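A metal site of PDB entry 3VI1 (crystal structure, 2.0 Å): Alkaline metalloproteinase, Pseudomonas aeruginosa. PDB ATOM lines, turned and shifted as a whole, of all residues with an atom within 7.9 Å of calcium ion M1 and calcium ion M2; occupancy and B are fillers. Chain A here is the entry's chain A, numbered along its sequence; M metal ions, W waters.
N of Gly 288 is in hydrogen-bond range of O of Thr 254 (3.3 Å).
OD2 of Asp 285 sits close to OH of Tyr 259, 2.6 Å away.
The backbone carbonyl oxygen of Asp 290 lies within hydrogen-bond range of the backbone NH of Asn 330.
O of Thr 257 is in hydrogen-bond range of N of Thr 291.
O of Trp 284 sits at hydrogen-bond distance from NH2 of Arg 253, 2.9 Å away.
The guanidinium group (NE) of Arg 253 is in hydrogen-bond range of the side-chain hydroxyl (OH) of Tyr 259 (3.2 Å).
The nearest printed residue that does not touch calcium ion M1 is Gly 287 (4.03 Å).
Merely in contact with calcium ion M2: Thr 254 (3.96 Å).
Within 4 Å of calcium ion M2: Arg 253, Thr 254, Gly 255, Thr 257, Asp 285, Gly 287 and Asp 290.
The nearest printed residue that does not touch calcium ion M2 is Gly 288 (4.4 Å).
Calcium ion M1 is bound by O of Thr 327 (2.4 Å), water W2 (2.4 Å), water W1 (2.4 Å), OD2 of Asp 290 (2.4 Å), O of Gly 288 (2.4 Å), OE1 of Glu 329 (2.6 Å) and OE2 of Glu 329 (2.8 Å).
Calcium ion M1 has seven donor atoms within binding distance.
Calcium ion M2 is bound by the backbone carbonyl oxygen (O) of Gly 287, at 2.3 Å.
O of Arg 253 is bound to calcium ion M2 (2.3 Å).
The backbone carbonyl oxygen (O) of Gly 255 is bound to calcium ion M2 (2.4 Å).
OD1 of Asp 285 is bound to calcium ion M2, 2.4 Å away.
Calcium ion M2 is bound by OD1 of Asp 290 (2.5 Å).
Calcium ion M2 is bound by OG1 of Thr 257, 2.6 Å away.
Calcium ion M2 is bound by OD2 of Asp 285, at 2.8 Å.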
ATOM      1  N   THR A 252      10.485 -32.609 -20.527  1.00  0.00           N
ATOM      2  CA  THR A 252       9.439 -32.793 -21.530  1.00  0.00           C
ATOM      3  C   THR A 252       9.869 -32.332 -22.926  1.00  0.00           C
ATOM      4  O   THR A 252      10.227 -31.175 -23.120  1.00  0.00           O
ATOM      5  CB  THR A 252       8.133 -32.090 -21.109  1.00  0.00           C
ATOM      6  OG1 THR A 252       7.764 -32.509 -19.787  1.00  0.00           O
ATOM      7  CG2 THR A 252       6.999 -32.412 -22.061  1.00  0.00           C
ATOM      8  N   ARG A 253       9.800 -33.254 -23.886  1.00  0.00           N
ATOM      9  CA  ARG A 253      10.119 -32.985 -25.289  1.00  0.00           C
ATOM     10  C   ARG A 253      11.436 -32.222 -25.455  1.00  0.00           C
ATOM     11  O   ARG A 253      11.464 -31.128 -26.021  1.00  0.00           O
ATOM     12  CB  ARG A 253       8.959 -32.239 -25.962  1.00  0.00           C
ATOM     13  CG  ARG A 253       7.659 -33.030 -26.048  1.00  0.00           C
ATOM     14  CD  ARG A 253       6.521 -32.191 -26.618  1.00  0.00           C
ATOM     15  NE  ARG A 253       6.024 -31.208 -25.654  1.00  0.00           N
ATOM     16  CZ  ARG A 253       4.996 -31.402 -24.838  1.00  0.00           C
ATOM     17  NH1 ARG A 253       4.334 -32.551 -24.847  1.00  0.00           N
ATOM     18  NH2 ARG A 253       4.623 -30.436 -24.008  1.00  0.00           N
ATOM     19  N   THR A 254      12.511 -32.813 -24.948  1.00  0.00           N
ATOM     20  CA  THR A 254      13.838 -32.189 -24.988  1.00  0.00           C
ATOM     21  C   THR A 254      14.520 -32.324 -26.351  1.00  0.00           C
ATOM     22  O   THR A 254      15.492 -31.619 -26.641  1.00  0.00           O
ATOM     23  CB  THR A 254      14.773 -32.738 -23.887  1.00  0.00           C
ATOM     24  OG1 THR A 254      14.816 -34.161 -23.952  1.00  0.00           O
ATOM     25  CG2 THR A 254      14.276 -32.313 -22.509  1.00  0.00           C
ATOM     26  N   GLY A 255      14.018 -33.238 -27.187  1.00  0.00           N
ATOM     27  CA  GLY A 255      14.530 -33.432 -28.530  1.00  0.00           C
ATOM     28  C   GLY A 255      13.871 -32.497 -29.534  1.00  0.00           C
ATOM     29  O   GLY A 255      13.123 -31.599 -29.145  1.00  0.00           O
ATOM     30  N   ASP A 256      14.161 -32.703 -30.818  1.00  0.00           N
ATOM     31  CA  ASP A 256      13.589 -31.899 -31.887  1.00  0.00           C
ATOM     32  C   ASP A 256      12.101 -32.200 -32.049  1.00  0.00           C
ATOM     33  O   ASP A 256      11.727 -33.317 -32.417  1.00  0.00           O
ATOM     34  CB  ASP A 256      14.348 -32.119 -33.198  1.00  0.00           C
ATOM     35  CG  ASP A 256      15.724 -31.446 -33.214  1.00  0.00           C
ATOM     36  OD1 ASP A 256      16.187 -31.008 -32.139  1.00  0.00           O
ATOM     37  OD2 ASP A 256      16.329 -31.373 -34.302  1.00  0.00           O
ATOM     38  N   THR A 257      11.265 -31.206 -31.764  1.00  0.00           N
ATOM     39  CA  THR A 257       9.824 -31.390 -31.707  1.00  0.00           C
ATOM     40  C   THR A 257       9.086 -30.554 -32.748  1.00  0.00           C
ATOM     41  O   THR A 257       9.311 -29.348 -32.870  1.00  0.00           O
ATOM     42  CB  THR A 257       9.266 -31.046 -30.302  1.00  0.00           C
ATOM     43  OG1 THR A 257      10.182 -31.467 -29.299  1.00  0.00           O
ATOM     44  CG2 THR A 257       7.921 -31.727 -30.081  1.00  0.00           C
ATOM     45  N   VAL A 258       8.209 -31.210 -33.500  1.00  0.00           N
ATOM     46  CA  VAL A 258       7.399 -30.534 -34.503  1.00  0.00           C
ATOM     47  C   VAL A 258       5.948 -30.421 -34.020  1.00  0.00           C
ATOM     48  O   VAL A 258       5.340 -31.421 -33.626  1.00  0.00           O
ATOM     49  CB  VAL A 258       7.458 -31.252 -35.884  1.00  0.00           C
ATOM     50  CG1 VAL A 258       6.646 -30.492 -36.929  1.00  0.00           C
ATOM     51  CG2 VAL A 258       8.907 -31.387 -36.344  1.00  0.00           C
ATOM     52  N   TYR A 259       5.427 -29.205 -34.034  1.00  0.00           N
ATOM     53  CA  TYR A 259       4.056 -28.928 -33.625  1.00  0.00           C
ATOM     54  C   TYR A 259       3.201 -28.568 -34.831  1.00  0.00           C
ATOM     55  O   TYR A 259       3.680 -27.956 -35.783  1.00  0.00           O
ATOM     56  CB  TYR A 259       4.027 -27.794 -32.594  1.00  0.00           C
ATOM     57  CG  TYR A 259       4.768 -28.112 -31.313  1.00  0.00           C
ATOM     58  CD1 TYR A 259       6.143 -27.896 -31.208  1.00  0.00           C
ATOM     59  CD2 TYR A 259       4.089 -28.621 -30.208  1.00  0.00           C
ATOM     60  CE1 TYR A 259       6.828 -28.200 -30.028  1.00  0.00           C
ATOM     61  CE2 TYR A 259       4.767 -28.915 -29.022  1.00  0.00           C
ATOM     62  CZ  TYR A 259       6.136 -28.697 -28.947  1.00  0.00           C
ATOM     63  OH  TYR A 259       6.796 -28.991 -27.785  1.00  0.00           O
ATOM     64  N   ASN A 264       5.401 -34.921 -33.938  1.00  0.00           N
ATOM     65  CA  ASN A 264       5.989 -36.055 -33.221  1.00  0.00           C
ATOM     66  C   ASN A 264       5.758 -35.967 -31.713  1.00  0.00           C
ATOM     67  O   ASN A 264       6.404 -36.672 -30.929  1.00  0.00           O
ATOM     68  CB  ASN A 264       7.492 -36.163 -33.533  1.00  0.00           C
ATOM     69  CG  ASN A 264       8.294 -34.975 -32.988  1.00  0.00           C
ATOM     70  OD1 ASN A 264       7.782 -33.854 -32.894  1.00  0.00           O
ATOM     71  ND2 ASN A 264       9.545 -35.230 -32.642  1.00  0.00           N
ATOM     72  N   VAL A 283       2.429 -23.976 -26.416  1.00  0.00           N
ATOM     73  CA  VAL A 283       3.613 -24.842 -26.489  1.00  0.00           C
ATOM     74  C   VAL A 283       4.453 -24.788 -25.210  1.00  0.00           C
ATOM     75  O   VAL A 283       5.011 -23.741 -24.877  1.00  0.00           O
ATOM     76  CB  VAL A 283       4.523 -24.471 -27.691  1.00  0.00           C
ATOM     77  CG1 VAL A 283       5.743 -25.374 -27.749  1.00  0.00           C
ATOM     78  CG2 VAL A 283       3.750 -24.531 -28.997  1.00  0.00           C
ATOM     79  N   TRP A 284       4.524 -25.905 -24.501  1.00  0.00           N
ATOM     80  CA  TRP A 284       5.555 -26.098 -23.487  1.00  0.00           C
ATOM     81  C   TRP A 284       6.614 -27.045 -24.026  1.00  0.00           C
ATOM     82  O   TRP A 284       6.318 -28.173 -24.434  1.00  0.00           O
ATOM     83  CB  TRP A 284       5.002 -26.616 -22.158  1.00  0.00           C
ATOM     84  CG  TRP A 284       6.111 -26.989 -21.213  1.00  0.00           C
ATOM     85  CD1 TRP A 284       6.481 -28.247 -20.836  1.00  0.00           C
ATOM     86  CD2 TRP A 284       7.027 -26.091 -20.560  1.00  0.00           C
ATOM     87  NE1 TRP A 284       7.549 -28.198 -19.978  1.00  0.00           N
ATOM     88  CE2 TRP A 284       7.911 -26.888 -19.790  1.00  0.00           C
ATOM     89  CE3 TRP A 284       7.187 -24.701 -20.547  1.00  0.00           C
ATOM     90  CZ2 TRP A 284       8.940 -26.334 -19.018  1.00  0.00           C
ATOM     91  CZ3 TRP A 284       8.201 -24.156 -19.776  1.00  0.00           C
ATOM     92  CH2 TRP A 284       9.070 -24.970 -19.028  1.00  0.00           C
ATOM     93  N   ASP A 285       7.862 -26.571 -24.036  1.00  0.00           N
ATOM     94  CA  ASP A 285       8.960 -27.314 -24.636  1.00  0.00           C
ATOM     95  C   ASP A 285      10.268 -27.024 -23.903  1.00  0.00           C
ATOM     96  O   ASP A 285      10.649 -25.861 -23.744  1.00  0.00           O
ATOM     97  CB  ASP A 285       9.083 -26.942 -26.121  1.00  0.00           C
ATOM     98  CG  ASP A 285       9.913 -27.922 -26.901  1.00  0.00           C
ATOM     99  OD1 ASP A 285      11.117 -28.051 -26.613  1.00  0.00           O
ATOM    100  OD2 ASP A 285       9.364 -28.566 -27.828  1.00  0.00           O
ATOM    101  N   ALA A 286      10.940 -28.085 -23.460  1.00  0.00           N
ATOM    102  CA  ALA A 286      12.112 -27.964 -22.588  1.00  0.00           C
ATOM    103  C   ALA A 286      13.440 -27.726 -23.313  1.00  0.00           C
ATOM    104  O   ALA A 286      14.356 -27.144 -22.729  1.00  0.00           O
ATOM    105  CB  ALA A 286      12.217 -29.191 -21.688  1.00  0.00           C
ATOM    106  N   GLY A 287      13.560 -28.189 -24.549  1.00  0.00           N
ATOM    107  CA  GLY A 287      14.804 -28.031 -25.299  1.00  0.00           C
ATOM    108  C   GLY A 287      14.781 -28.592 -26.717  1.00  0.00           C
ATOM    109  O   GLY A 287      13.780 -29.165 -27.155  1.00  0.00           O
ATOM    110  N   GLY A 288      15.903 -28.420 -27.420  1.00  0.00           N
ATOM    111  CA  GLY A 288      16.046 -28.927 -28.778  1.00  0.00           C
ATOM    112  C   GLY A 288      15.653 -27.929 -29.846  1.00  0.00           C
ATOM    113  O   GLY A 288      15.258 -26.790 -29.539  1.00  0.00           O
ATOM    114  N   ASN A 289      15.764 -28.344 -31.102  1.00  0.00           N
ATOM    115  CA  ASN A 289      15.409 -27.525 -32.259  1.00  0.00           C
ATOM    116  C   ASN A 289      13.963 -27.788 -32.661  1.00  0.00           C
ATOM    117  O   ASN A 289      13.635 -28.866 -33.155  1.00  0.00           O
ATOM    118  CB  ASN A 289      16.361 -27.829 -33.418  1.00  0.00           C
ATOM    119  CG  ASN A 289      16.254 -26.823 -34.544  1.00  0.00           C
ATOM    120  OD1 ASN A 289      16.534 -25.631 -34.357  1.00  0.00           O
ATOM    121  ND2 ASN A 289      15.869 -27.295 -35.720  1.00  0.00           N
ATOM    122  N   ASP A 290      13.105 -26.802 -32.464  1.00  0.00           N
ATOM    123  CA  ASP A 290      11.662 -27.021 -32.562  1.00  0.00           C
ATOM    124  C   ASP A 290      10.981 -26.233 -33.671  1.00  0.00           C
ATOM    125  O   ASP A 290      11.398 -25.120 -34.012  1.00  0.00           O
ATOM    126  CB  ASP A 290      11.002 -26.734 -31.215  1.00  0.00           C
ATOM    127  CG  ASP A 290      11.675 -27.479 -30.075  1.00  0.00           C
ATOM    128  OD1 ASP A 290      11.796 -28.721 -30.158  1.00  0.00           O
ATOM    129  OD2 ASP A 290      12.102 -26.822 -29.100  1.00  0.00           O
ATOM    130  N   THR A 291       9.937 -26.829 -34.249  1.00  0.00           N
ATOM    131  CA  THR A 291       9.275 -26.281 -35.423  1.00  0.00           C
ATOM    132  C   THR A 291       7.755 -26.201 -35.282  1.00  0.00           C
ATOM    133  O   THR A 291       7.105 -27.168 -34.882  1.00  0.00           O
ATOM    134  CB  THR A 291       9.624 -27.102 -36.689  1.00  0.00           C
ATOM    135  OG1 THR A 291      11.044 -27.232 -36.810  1.00  0.00           O
ATOM    136  CG2 THR A 291       9.077 -26.443 -37.951  1.00  0.00           C
ATOM    137  N   VAL A 326       9.938 -20.668 -23.028  1.00  0.00           N
ATOM    138  CA  VAL A 326      10.065 -21.637 -24.110  1.00  0.00           C
ATOM    139  C   VAL A 326      10.670 -20.993 -25.363  1.00  0.00           C
ATOM    140  O   VAL A 326      10.213 -19.938 -25.800  1.00  0.00           O
ATOM    141  CB  VAL A 326       8.712 -22.291 -24.471  1.00  0.00           C
ATOM    142  CG1 VAL A 326       8.859 -23.270 -25.636  1.00  0.00           C
ATOM    143  CG2 VAL A 326       8.116 -22.986 -23.270  1.00  0.00           C
ATOM    144  N   THR A 327      11.693 -21.635 -25.916  1.00  0.00           N
ATOM    145  CA  THR A 327      12.324 -21.185 -27.151  1.00  0.00           C
ATOM    146  C   THR A 327      11.963 -22.120 -28.311  1.00  0.00           C
ATOM    147  O   THR A 327      12.383 -23.279 -28.342  1.00  0.00           O
ATOM    148  CB  THR A 327      13.863 -21.060 -27.012  1.00  0.00           C
ATOM    149  OG1 THR A 327      14.173 -20.295 -25.839  1.00  0.00           O
ATOM    150  CG2 THR A 327      14.469 -20.377 -28.233  1.00  0.00           C
ATOM    151  N   VAL A 328      11.164 -21.601 -29.243  1.00  0.00           N
ATOM    152  CA  VAL A 328      10.819 -22.314 -30.475  1.00  0.00           C
ATOM    153  C   VAL A 328      11.624 -21.706 -31.629  1.00  0.00           C
ATOM    154  O   VAL A 328      11.642 -20.490 -31.805  1.00  0.00           O
ATOM    155  CB  VAL A 328       9.296 -22.251 -30.783  1.00  0.00           C
ATOM    156  CG1 VAL A 328       8.958 -23.060 -32.035  1.00  0.00           C
ATOM    157  CG2 VAL A 328       8.488 -22.750 -29.595  1.00  0.00           C
ATOM    158  N   GLU A 329      12.293 -22.564 -32.388  1.00  0.00           N
ATOM    159  CA  GLU A 329      13.260 -22.112 -33.381  1.00  0.00           C
ATOM    160  C   GLU A 329      12.677 -21.847 -34.767  1.00  0.00           C
ATOM    161  O   GLU A 329      13.007 -20.843 -35.396  1.00  0.00           O
ATOM    162  CB  GLU A 329      14.414 -23.120 -33.504  1.00  0.00           C
ATOM    163  CG  GLU A 329      15.400 -23.098 -32.333  1.00  0.00           C
ATOM    164  CD  GLU A 329      14.819 -23.644 -31.041  1.00  0.00           C
ATOM    165  OE1 GLU A 329      13.902 -24.496 -31.083  1.00  0.00           O
ATOM    166  OE2 GLU A 329      15.287 -23.239 -29.949  1.00  0.00           O
ATOM    167  N   ASN A 330      11.822 -22.743 -35.248  1.00  0.00           N
ATOM    168  CA  ASN A 330      11.410 -22.735 -36.650  1.00  0.00           C
ATOM    169  C   ASN A 330       9.906 -22.593 -36.869  1.00  0.00           C
ATOM    170  O   ASN A 330       9.106 -23.020 -36.036  1.00  0.00           O
ATOM    171  CB  ASN A 330      11.932 -23.983 -37.362  1.00  0.00           C
ATOM    172  CG  ASN A 330      13.359 -24.326 -36.973  1.00  0.00           C
ATOM    173  OD1 ASN A 330      14.247 -23.479 -36.977  1.00  0.00           O
ATOM    174  ND2 ASN A 330      13.587 -25.602 -36.640  1.00  0.00           N
ATOM    175  N   VAL A 345      16.832 -15.827 -31.273  1.00  0.00           N
ATOM    176  CA  VAL A 345      17.819 -16.827 -31.710  1.00  0.00           C
ATOM    177  C   VAL A 345      17.735 -17.097 -33.222  1.00  0.00           C
ATOM    178  O   VAL A 345      16.910 -16.500 -33.920  1.00  0.00           O
ATOM    179  CB  VAL A 345      17.696 -18.167 -30.909  1.00  0.00           C
ATOM    180  CG1 VAL A 345      17.910 -17.937 -29.421  1.00  0.00           C
ATOM    181  CG2 VAL A 345      16.364 -18.865 -31.171  1.00  0.00           C
HETATM  182 CA    CA M   1      13.756 -25.188 -28.619  1.00  0.00          CA
HETATM  183 CA    CA M   2      11.798 -29.958 -27.991  1.00  0.00          CA
HETATM  184  O   HOH W   1      15.474 -24.453 -27.154  1.00  0.00           O
HETATM  185  O   HOH W   2      12.636 -25.882 -26.647  1.00  0.00           O
